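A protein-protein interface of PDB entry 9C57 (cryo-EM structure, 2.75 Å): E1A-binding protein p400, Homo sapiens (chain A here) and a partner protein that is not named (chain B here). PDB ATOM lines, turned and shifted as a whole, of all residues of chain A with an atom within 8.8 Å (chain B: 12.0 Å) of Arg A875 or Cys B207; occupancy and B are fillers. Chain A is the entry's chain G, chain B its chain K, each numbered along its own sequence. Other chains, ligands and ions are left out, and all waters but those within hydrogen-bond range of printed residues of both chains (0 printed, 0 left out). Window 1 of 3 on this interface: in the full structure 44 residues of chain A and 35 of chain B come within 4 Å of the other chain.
Of the 16 printed residues of chain A, 2 touch a printed residue of chain B. Among the printed residues, 3 pairs touch across the chains. Among the printed residues, no Asp or Glu carboxylate lies within 4 Å of a Lys or Arg side-chain nitrogen of the other chain.
Lys B206 touches Arg A875 (C to NH2, 3.8 Å). OG of Ser A882 touches CE of Lys B204 (3.4 Å).
The guanidinium group (NH2) of Arg A875 lies close to the backbone NH (N) of Cys B207 (2.8 Å).
No residue of chain B comes within 4 Å of Ala A871. Thr A873 touches none of the printed residues of chain B. Arg A875 touches just these residues of chain B: Lys B206 and Cys B207. No residue of chain B comes within 4 Å of Cys A879. Of the printed residues of chain B, Ser A882 touches Lys B204 (3.4 Å). Of the printed residues of chain A, Lys B204 touches Ser A882 (3.4 Å). Printed residues of chain A within 4 Å of Lys B206: Arg A875 (3.8 Å). Of chain A, only Arg A875 comes within 4 Å of Cys B207. No residue of chain A comes within 4 Å of Gly B209.
NH1 of Arg A875 lies within salt-bridge range of OE1 of Glu A876 (3.1 Å). The backbone NH (N) of Gly B209 sits close to the side-chain sulfur (SG) of Cys B207 (3.0 Å).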
ATOM      1  N   ARG A 867     -21.721 -26.890 -15.232  1.00  0.00           N
ATOM      2  CA  ARG A 867     -21.405 -28.217 -15.745  1.00  0.00           C
ATOM      3  C   ARG A 867     -20.878 -28.145 -17.174  1.00  0.00           C
ATOM      4  O   ARG A 867     -19.945 -28.868 -17.536  1.00  0.00           O
ATOM      5  CB  ARG A 867     -22.640 -29.111 -15.670  1.00  0.00           C
ATOM      6  CG  ARG A 867     -22.391 -30.548 -16.085  1.00  0.00           C
ATOM      7  CD  ARG A 867     -21.248 -31.157 -15.302  1.00  0.00           C
ATOM      8  NE  ARG A 867     -21.216 -32.608 -15.415  1.00  0.00           N
ATOM      9  CZ  ARG A 867     -21.950 -33.432 -14.681  1.00  0.00           C
ATOM     10  NH1 ARG A 867     -22.782 -32.979 -13.757  1.00  0.00           N
ATOM     11  NH2 ARG A 867     -21.845 -34.741 -14.878  1.00  0.00           N
ATOM     12  N   ARG A 868     -21.458 -27.274 -18.001  1.00  0.00           N
ATOM     13  CA  ARG A 868     -20.996 -27.143 -19.378  1.00  0.00           C
ATOM     14  C   ARG A 868     -19.634 -26.471 -19.455  1.00  0.00           C
ATOM     15  O   ARG A 868     -18.844 -26.794 -20.343  1.00  0.00           O
ATOM     16  CB  ARG A 868     -22.016 -26.368 -20.211  1.00  0.00           C
ATOM     17  CG  ARG A 868     -23.229 -27.191 -20.599  1.00  0.00           C
ATOM     18  CD  ARG A 868     -24.108 -26.471 -21.602  1.00  0.00           C
ATOM     19  NE  ARG A 868     -25.013 -25.527 -20.957  1.00  0.00           N
ATOM     20  CZ  ARG A 868     -24.779 -24.230 -20.819  1.00  0.00           C
ATOM     21  NH1 ARG A 868     -23.659 -23.677 -21.258  1.00  0.00           N
ATOM     22  NH2 ARG A 868     -25.690 -23.468 -20.226  1.00  0.00           N
ATOM     23  N   ILE A 869     -19.337 -25.538 -18.550  1.00  0.00           N
ATOM     24  CA  ILE A 869     -17.992 -24.969 -18.511  1.00  0.00           C
ATOM     25  C   ILE A 869     -16.979 -26.045 -18.134  1.00  0.00           C
ATOM     26  O   ILE A 869     -15.891 -26.137 -18.724  1.00  0.00           O
ATOM     27  CB  ILE A 869     -17.943 -23.776 -17.540  1.00  0.00           C
ATOM     28  CG1 ILE A 869     -18.720 -22.596 -18.120  1.00  0.00           C
ATOM     29  CG2 ILE A 869     -16.505 -23.368 -17.274  1.00  0.00           C
ATOM     30  CD1 ILE A 869     -19.126 -21.571 -17.090  1.00  0.00           C
ATOM     31  N   ALA A 870     -17.323 -26.875 -17.148  1.00  0.00           N
ATOM     32  CA  ALA A 870     -16.463 -28.000 -16.796  1.00  0.00           C
ATOM     33  C   ALA A 870     -16.278 -28.937 -17.982  1.00  0.00           C
ATOM     34  O   ALA A 870     -15.174 -29.439 -18.226  1.00  0.00           O
ATOM     35  CB  ALA A 870     -17.053 -28.756 -15.608  1.00  0.00           C
ATOM     36  N   ALA A 871     -17.355 -29.199 -18.721  1.00  0.00           N
ATOM     37  CA  ALA A 871     -17.256 -30.066 -19.886  1.00  0.00           C
ATOM     38  C   ALA A 871     -16.362 -29.453 -20.953  1.00  0.00           C
ATOM     39  O   ALA A 871     -15.553 -30.152 -21.566  1.00  0.00           O
ATOM     40  CB  ALA A 871     -18.647 -30.345 -20.448  1.00  0.00           C
ATOM     41  N   SER A 872     -16.486 -28.145 -21.181  1.00  0.00           N
ATOM     42  CA  SER A 872     -15.662 -27.484 -22.189  1.00  0.00           C
ATOM     43  C   SER A 872     -14.185 -27.546 -21.824  1.00  0.00           C
ATOM     44  O   SER A 872     -13.335 -27.799 -22.688  1.00  0.00           O
ATOM     45  CB  SER A 872     -16.111 -26.034 -22.359  1.00  0.00           C
ATOM     46  OG  SER A 872     -15.330 -25.371 -23.336  1.00  0.00           O
ATOM     47  N   THR A 873     -13.851 -27.327 -20.549  1.00  0.00           N
ATOM     48  CA  THR A 873     -12.451 -27.439 -20.150  1.00  0.00           C
ATOM     49  C   THR A 873     -11.931 -28.872 -20.217  1.00  0.00           C
ATOM     50  O   THR A 873     -10.832 -29.095 -20.745  1.00  0.00           O
ATOM     51  CB  THR A 873     -12.236 -26.881 -18.741  1.00  0.00           C
ATOM     52  OG1 THR A 873     -10.858 -27.030 -18.378  1.00  0.00           O
ATOM     53  CG2 THR A 873     -13.095 -27.583 -17.722  1.00  0.00           C
ATOM     54  N   ALA A 874     -12.680 -29.844 -19.698  1.00  0.00           N
ATOM     55  CA  ALA A 874     -12.261 -31.233 -19.805  1.00  0.00           C
ATOM     56  C   ALA A 874     -12.122 -31.658 -21.251  1.00  0.00           C
ATOM     57  O   ALA A 874     -11.260 -32.475 -21.579  1.00  0.00           O
ATOM     58  CB  ALA A 874     -13.261 -32.149 -19.098  1.00  0.00           C
ATOM     59  N   ARG A 875     -12.938 -31.081 -22.123  1.00  0.00           N
ATOM     60  CA  ARG A 875     -12.923 -31.451 -23.526  1.00  0.00           C
ATOM     61  C   ARG A 875     -11.742 -30.801 -24.244  1.00  0.00           C
ATOM     62  O   ARG A 875     -11.157 -31.387 -25.161  1.00  0.00           O
ATOM     63  CB  ARG A 875     -14.269 -31.061 -24.134  1.00  0.00           C
ATOM     64  CG  ARG A 875     -14.348 -31.211 -25.600  1.00  0.00           C
ATOM     65  CD  ARG A 875     -14.045 -29.924 -26.281  1.00  0.00           C
ATOM     66  NE  ARG A 875     -13.741 -30.215 -27.666  1.00  0.00           N
ATOM     67  CZ  ARG A 875     -13.059 -29.415 -28.466  1.00  0.00           C
ATOM     68  NH1 ARG A 875     -12.692 -28.201 -28.086  1.00  0.00           N
ATOM     69  NH2 ARG A 875     -12.701 -29.858 -29.659  1.00  0.00           N
ATOM     70  N   GLU A 876     -11.355 -29.597 -23.815  1.00  0.00           N
ATOM     71  CA  GLU A 876     -10.108 -29.006 -24.293  1.00  0.00           C
ATOM     72  C   GLU A 876      -8.905 -29.849 -23.886  1.00  0.00           C
ATOM     73  O   GLU A 876      -7.992 -30.083 -24.692  1.00  0.00           O
ATOM     74  CB  GLU A 876      -9.964 -27.584 -23.751  1.00  0.00           C
ATOM     75  CG  GLU A 876      -8.986 -26.725 -24.523  1.00  0.00           C
ATOM     76  CD  GLU A 876      -9.459 -26.420 -25.925  1.00  0.00           C
ATOM     77  OE1 GLU A 876     -10.598 -26.802 -26.265  1.00  0.00           O
ATOM     78  OE2 GLU A 876      -8.693 -25.794 -26.686  1.00  0.00           O
ATOM     79  N   ILE A 877      -8.877 -30.310 -22.634  1.00  0.00           N
ATOM     80  CA  ILE A 877      -7.818 -31.224 -22.217  1.00  0.00           C
ATOM     81  C   ILE A 877      -7.852 -32.529 -22.994  1.00  0.00           C
ATOM     82  O   ILE A 877      -6.792 -33.077 -23.315  1.00  0.00           O
ATOM     83  CB  ILE A 877      -7.887 -31.515 -20.704  1.00  0.00           C
ATOM     84  CG1 ILE A 877      -7.249 -30.369 -19.917  1.00  0.00           C
ATOM     85  CG2 ILE A 877      -7.175 -32.820 -20.371  1.00  0.00           C
ATOM     86  CD1 ILE A 877      -8.111 -29.144 -19.791  1.00  0.00           C
ATOM     87  N   GLU A 878      -9.041 -33.043 -23.301  1.00  0.00           N
ATOM     88  CA  GLU A 878      -9.149 -34.229 -24.139  1.00  0.00           C
ATOM     89  C   GLU A 878      -8.559 -33.985 -25.522  1.00  0.00           C
ATOM     90  O   GLU A 878      -7.890 -34.859 -26.073  1.00  0.00           O
ATOM     91  CB  GLU A 878     -10.611 -34.652 -24.259  1.00  0.00           C
ATOM     92  CG  GLU A 878     -11.060 -35.616 -23.186  1.00  0.00           C
ATOM     93  CD  GLU A 878     -12.463 -36.123 -23.423  1.00  0.00           C
ATOM     94  OE1 GLU A 878     -13.146 -35.580 -24.315  1.00  0.00           O
ATOM     95  OE2 GLU A 878     -12.884 -37.064 -22.718  1.00  0.00           O
ATOM     96  N   CYS A 879      -8.813 -32.811 -26.100  1.00  0.00           N
ATOM     97  CA  CYS A 879      -8.211 -32.477 -27.387  1.00  0.00           C
ATOM     98  C   CYS A 879      -6.692 -32.427 -27.281  1.00  0.00           C
ATOM     99  O   CYS A 879      -5.981 -32.899 -28.177  1.00  0.00           O
ATOM    100  CB  CYS A 879      -8.760 -31.142 -27.890  1.00  0.00           C
ATOM    101  SG  CYS A 879      -8.380 -30.786 -29.617  1.00  0.00           S
ATOM    102  N   PHE A 880      -6.176 -31.860 -26.190  1.00  0.00           N
ATOM    103  CA  PHE A 880      -4.731 -31.851 -25.973  1.00  0.00           C
ATOM    104  C   PHE A 880      -4.171 -33.270 -25.924  1.00  0.00           C
ATOM    105  O   PHE A 880      -3.148 -33.575 -26.551  1.00  0.00           O
ATOM    106  CB  PHE A 880      -4.410 -31.098 -24.682  1.00  0.00           C
ATOM    107  CG  PHE A 880      -3.097 -31.486 -24.061  1.00  0.00           C
ATOM    108  CD1 PHE A 880      -1.918 -30.895 -24.476  1.00  0.00           C
ATOM    109  CD2 PHE A 880      -3.047 -32.427 -23.048  1.00  0.00           C
ATOM    110  CE1 PHE A 880      -0.717 -31.246 -23.902  1.00  0.00           C
ATOM    111  CE2 PHE A 880      -1.846 -32.779 -22.472  1.00  0.00           C
ATOM    112  CZ  PHE A 880      -0.682 -32.188 -22.899  1.00  0.00           C
ATOM    113  N   TRP A 881      -4.841 -34.159 -25.189  1.00  0.00           N
ATOM    114  CA  TRP A 881      -4.351 -35.526 -25.070  1.00  0.00           C
ATOM    115  C   TRP A 881      -4.497 -36.296 -26.374  1.00  0.00           C
ATOM    116  O   TRP A 881      -3.681 -37.171 -26.663  1.00  0.00           O
ATOM    117  CB  TRP A 881      -5.077 -36.239 -23.934  1.00  0.00           C
ATOM    118  CG  TRP A 881      -4.470 -35.948 -22.602  1.00  0.00           C
ATOM    119  CD1 TRP A 881      -4.913 -35.049 -21.683  1.00  0.00           C
ATOM    120  CD2 TRP A 881      -3.306 -36.560 -22.037  1.00  0.00           C
ATOM    121  NE1 TRP A 881      -4.097 -35.057 -20.579  1.00  0.00           N
ATOM    122  CE2 TRP A 881      -3.103 -35.978 -20.771  1.00  0.00           C
ATOM    123  CE3 TRP A 881      -2.416 -37.542 -22.478  1.00  0.00           C
ATOM    124  CZ2 TRP A 881      -2.049 -36.346 -19.943  1.00  0.00           C
ATOM    125  CZ3 TRP A 881      -1.369 -37.905 -21.653  1.00  0.00           C
ATOM    126  CH2 TRP A 881      -1.194 -37.308 -20.401  1.00  0.00           C
ATOM    127  N   SER A 882      -5.505 -35.977 -27.185  1.00  0.00           N
ATOM    128  CA  SER A 882      -5.621 -36.606 -28.497  1.00  0.00           C
ATOM    129  C   SER A 882      -4.523 -36.123 -29.438  1.00  0.00           C
ATOM    130  O   SER A 882      -4.001 -36.900 -30.247  1.00  0.00           O
ATOM    131  CB  SER A 882      -6.997 -36.328 -29.094  1.00  0.00           C
ATOM    132  OG  SER A 882      -7.204 -37.103 -30.262  1.00  0.00           O
ATOM    133  N   LYS B 203     -13.472 -39.909 -36.483  1.00  0.00           N
ATOM    134  CA  LYS B 203     -12.808 -38.618 -36.374  1.00  0.00           C
ATOM    135  C   LYS B 203     -12.758 -38.154 -34.923  1.00  0.00           C
ATOM    136  O   LYS B 203     -13.609 -38.505 -34.101  1.00  0.00           O
ATOM    137  CB  LYS B 203     -13.532 -37.573 -37.223  1.00  0.00           C
ATOM    138  CG  LYS B 203     -13.524 -37.860 -38.717  1.00  0.00           C
ATOM    139  CD  LYS B 203     -12.125 -37.747 -39.301  1.00  0.00           C
ATOM    140  CE  LYS B 203     -12.167 -37.376 -40.775  1.00  0.00           C
ATOM    141  NZ  LYS B 203     -12.872 -38.400 -41.594  1.00  0.00           N
ATOM    142  N   LYS B 204     -11.741 -37.353 -34.615  1.00  0.00           N
ATOM    143  CA  LYS B 204     -11.552 -36.793 -33.284  1.00  0.00           C
ATOM    144  C   LYS B 204     -12.145 -35.394 -33.141  1.00  0.00           C
ATOM    145  O   LYS B 204     -11.904 -34.737 -32.123  1.00  0.00           O
ATOM    146  CB  LYS B 204     -10.058 -36.760 -32.942  1.00  0.00           C
ATOM    147  CG  LYS B 204      -9.305 -38.047 -33.269  1.00  0.00           C
ATOM    148  CD  LYS B 204      -9.880 -39.265 -32.557  1.00  0.00           C
ATOM    149  CE  LYS B 204      -9.745 -39.152 -31.047  1.00  0.00           C
ATOM    150  NZ  LYS B 204     -10.075 -40.432 -30.360  1.00  0.00           N
ATOM    151  N   ARG B 205     -12.895 -34.924 -34.140  1.00  0.00           N
ATOM    152  CA  ARG B 205     -13.586 -33.639 -34.083  1.00  0.00           C
ATOM    153  C   ARG B 205     -12.591 -32.484 -34.043  1.00  0.00           C
ATOM    154  O   ARG B 205     -12.425 -31.771 -35.038  1.00  0.00           O
ATOM    155  CB  ARG B 205     -14.523 -33.599 -32.872  1.00  0.00           C
ATOM    156  CG  ARG B 205     -15.614 -34.661 -32.934  1.00  0.00           C
ATOM    157  CD  ARG B 205     -16.520 -34.631 -31.715  1.00  0.00           C
ATOM    158  NE  ARG B 205     -17.263 -33.381 -31.611  1.00  0.00           N
ATOM    159  CZ  ARG B 205     -18.249 -33.027 -32.426  1.00  0.00           C
ATOM    160  NH1 ARG B 205     -18.644 -33.810 -33.416  1.00  0.00           N
ATOM    161  NH2 ARG B 205     -18.855 -31.859 -32.239  1.00  0.00           N
ATOM    162  N   LYS B 206     -11.923 -32.291 -32.907  1.00  0.00           N
ATOM    163  CA  LYS B 206     -10.775 -31.390 -32.805  1.00  0.00           C
ATOM    164  C   LYS B 206     -11.134 -29.945 -33.164  1.00  0.00           C
ATOM    165  O   LYS B 206     -10.717 -29.410 -34.193  1.00  0.00           O
ATOM    166  CB  LYS B 206      -9.625 -31.897 -33.677  1.00  0.00           C
ATOM    167  CG  LYS B 206      -8.999 -33.171 -33.164  1.00  0.00           C
ATOM    168  CD  LYS B 206      -7.634 -33.393 -33.777  1.00  0.00           C
ATOM    169  CE  LYS B 206      -6.565 -32.583 -33.060  1.00  0.00           C
ATOM    170  NZ  LYS B 206      -5.228 -32.729 -33.695  1.00  0.00           N
ATOM    171  N   CYS B 207     -11.979 -29.349 -32.317  1.00  0.00           N
ATOM    172  CA  CYS B 207     -12.087 -27.913 -32.027  1.00  0.00           C
ATOM    173  C   CYS B 207     -13.342 -27.270 -32.602  1.00  0.00           C
ATOM    174  O   CYS B 207     -14.234 -26.886 -31.834  1.00  0.00           O
ATOM    175  CB  CYS B 207     -10.864 -27.131 -32.528  1.00  0.00           C
ATOM    176  SG  CYS B 207     -11.191 -25.371 -32.774  1.00  0.00           S
ATOM    177  N   PRO B 208     -13.475 -27.167 -33.928  1.00  0.00           N
ATOM    178  CA  PRO B 208     -14.332 -26.130 -34.524  1.00  0.00           C
ATOM    179  C   PRO B 208     -14.903 -25.068 -33.585  1.00  0.00           C
ATOM    180  O   PRO B 208     -16.041 -24.631 -33.787  1.00  0.00           O
ATOM    181  CB  PRO B 208     -15.447 -26.967 -35.159  1.00  0.00           C
ATOM    182  CG  PRO B 208     -14.748 -28.292 -35.540  1.00  0.00           C
ATOM    183  CD  PRO B 208     -13.394 -28.319 -34.838  1.00  0.00           C
ATOM    184  N   GLY B 209     -14.139 -24.630 -32.581  1.00  0.00           N
ATOM    185  CA  GLY B 209     -14.576 -23.599 -31.666  1.00  0.00           C
ATOM    186  C   GLY B 209     -15.991 -23.807 -31.165  1.00  0.00           C
ATOM    187  O   GLY B 209     -16.478 -24.936 -31.067  1.00  0.00           O
ATOM    188  N   PRO B 210     -16.672 -22.717 -30.815  1.00  0.00           N
ATOM    189  CA  PRO B 210     -18.113 -22.806 -30.557  1.00  0.00           C
ATOM    190  C   PRO B 210     -18.857 -23.239 -31.808  1.00  0.00           C
ATOM    191  O   PRO B 210     -18.537 -22.816 -32.920  1.00  0.00           O
ATOM    192  CB  PRO B 210     -18.491 -21.384 -30.133  1.00  0.00           C
ATOM    193  CG  PRO B 210     -17.222 -20.766 -29.679  1.00  0.00           C
ATOM    194  CD  PRO B 210     -16.142 -21.378 -30.513  1.00  0.00           C
ATOM    195  N   ILE B 211     -19.868 -24.085 -31.621  1.00  0.00           N
ATOM    196  CA  ILE B 211     -20.551 -24.723 -32.736  1.00  0.00           C
ATOM    197  C   ILE B 211     -22.053 -24.737 -32.496  1.00  0.00           C
ATOM    198  O   ILE B 211     -22.526 -24.703 -31.355  1.00  0.00           O
ATOM    199  CB  ILE B 211     -20.034 -26.161 -32.969  1.00  0.00           C
ATOM    200  CG1 ILE B 211     -20.067 -26.959 -31.666  1.00  0.00           C
ATOM    201  CG2 ILE B 211     -18.628 -26.133 -33.535  1.00  0.00           C
ATOM    202  CD1 ILE B 211     -19.796 -28.428 -31.849  1.00  0.00           C
ATOM    203  N   ILE B 212     -22.803 -24.796 -33.593  1.00  0.00           N
ATOM    204  CA  ILE B 212     -24.246 -24.995 -33.574  1.00  0.00           C
ATOM    205  C   ILE B 212     -24.522 -26.320 -34.265  1.00  0.00           C
ATOM    206  O   ILE B 212     -24.198 -26.491 -35.446  1.00  0.00           O
ATOM    207  CB  ILE B 212     -24.998 -23.850 -34.268  1.00  0.00           C
ATOM    208  CG1 ILE B 212     -24.617 -22.506 -33.647  1.00  0.00           C
ATOM    209  CG2 ILE B 212     -26.499 -24.068 -34.171  1.00  0.00           C
ATOM    210  CD1 ILE B 212     -25.272 -21.322 -34.315  1.00  0.00           C
ATOM    211  N   THR B 213     -25.120 -27.253 -33.536  1.00  0.00           N
ATOM    212  CA  THR B 213     -25.389 -28.587 -34.048  1.00  0.00           C
ATOM    213  C   THR B 213     -26.846 -28.682 -34.472  1.00  0.00           C
ATOM    214  O   THR B 213     -27.744 -28.316 -33.709  1.00  0.00           O
ATOM    215  CB  THR B 213     -25.083 -29.649 -32.990  1.00  0.00           C
ATOM    216  OG1 THR B 213     -23.709 -29.554 -32.596  1.00  0.00           O
ATOM    217  CG2 THR B 213     -25.355 -31.041 -33.528  1.00  0.00           C
ATOM    218  N   THR B 267     -28.414 -27.714 -30.942  1.00  0.00           N
ATOM    219  CA  THR B 267     -27.560 -27.571 -29.772  1.00  0.00           C
ATOM    220  C   THR B 267     -26.618 -26.396 -29.973  1.00  0.00           C
ATOM    221  O   THR B 267     -25.971 -26.285 -31.019  1.00  0.00           O
ATOM    222  CB  THR B 267     -26.760 -28.851 -29.513  1.00  0.00           C
ATOM    223  OG1 THR B 267     -27.628 -29.986 -29.594  1.00  0.00           O
ATOM    224  CG2 THR B 267     -26.118 -28.811 -28.140  1.00  0.00           C
ATOM    225  N   PHE B 268     -26.555 -25.520 -28.977  1.00  0.00           N
ATOM    226  CA  PHE B 268     -25.602 -24.421 -28.942  1.00  0.00           C
ATOM    227  C   PHE B 268     -24.506 -24.763 -27.944  1.00  0.00           C
ATOM    228  O   PHE B 268     -24.794 -25.160 -26.811  1.00  0.00           O
ATOM    229  CB  PHE B 268     -26.282 -23.108 -28.554  1.00  0.00           C
ATOM    230  CG  PHE B 268     -27.328 -22.657 -29.526  1.00  0.00           C
ATOM    231  CD1 PHE B 268     -28.590 -23.221 -29.520  1.00  0.00           C
ATOM    232  CD2 PHE B 268     -27.053 -21.660 -30.442  1.00  0.00           C
ATOM    233  CE1 PHE B 268     -29.554 -22.802 -30.412  1.00  0.00           C
ATOM    234  CE2 PHE B 268     -28.014 -21.237 -31.334  1.00  0.00           C
ATOM    235  CZ  PHE B 268     -29.264 -21.810 -31.319  1.00  0.00           C
ATOM    236  N   SER B 269     -23.252 -24.617 -28.372  1.00  0.00           N
ATOM    237  CA  SER B 269     -22.136 -25.051 -27.539  1.00  0.00           C
ATOM    238  C   SER B 269     -22.072 -24.266 -26.235  1.00  0.00           C
ATOM    239  O   SER B 269     -21.928 -24.852 -25.158  1.00  0.00           O
ATOM    240  CB  SER B 269     -20.827 -24.910 -28.313  1.00  0.00           C
ATOM    241  OG  SER B 269     -19.787 -25.629 -27.680  1.00  0.00           O
ATOM    242  N   ASP B 270     -22.182 -22.943 -26.309  1.00  0.00           N
ATOM    243  CA  ASP B 270     -22.015 -22.091 -25.141  1.00  0.00           C
ATOM    244  C   ASP B 270     -23.149 -21.080 -25.084  1.00  0.00           C
ATOM    245  O   ASP B 270     -23.915 -20.914 -26.036  1.00  0.00           O
ATOM    246  CB  ASP B 270     -20.658 -21.380 -25.159  1.00  0.00           C
ATOM    247  CG  ASP B 270     -20.339 -20.773 -26.501  1.00  0.00           C
ATOM    248  OD1 ASP B 270     -21.180 -20.017 -27.028  1.00  0.00           O
ATOM    249  OD2 ASP B 270     -19.244 -21.049 -27.031  1.00  0.00           O
ATOM    250  N   THR B 273     -23.222 -17.809 -27.779  1.00  0.00           N
ATOM    251  CA  THR B 273     -23.886 -17.946 -29.070  1.00  0.00           C
ATOM    252  C   THR B 273     -25.392 -18.109 -28.906  1.00  0.00           C
ATOM    253  O   THR B 273     -26.163 -17.632 -29.748  1.00  0.00           O
ATOM    254  CB  THR B 273     -23.288 -19.122 -29.847  1.00  0.00           C
ATOM    255  OG1 THR B 273     -23.861 -19.176 -31.158  1.00  0.00           O
ATOM    256  CG2 THR B 273     -23.539 -20.436 -29.136  1.00  0.00           C
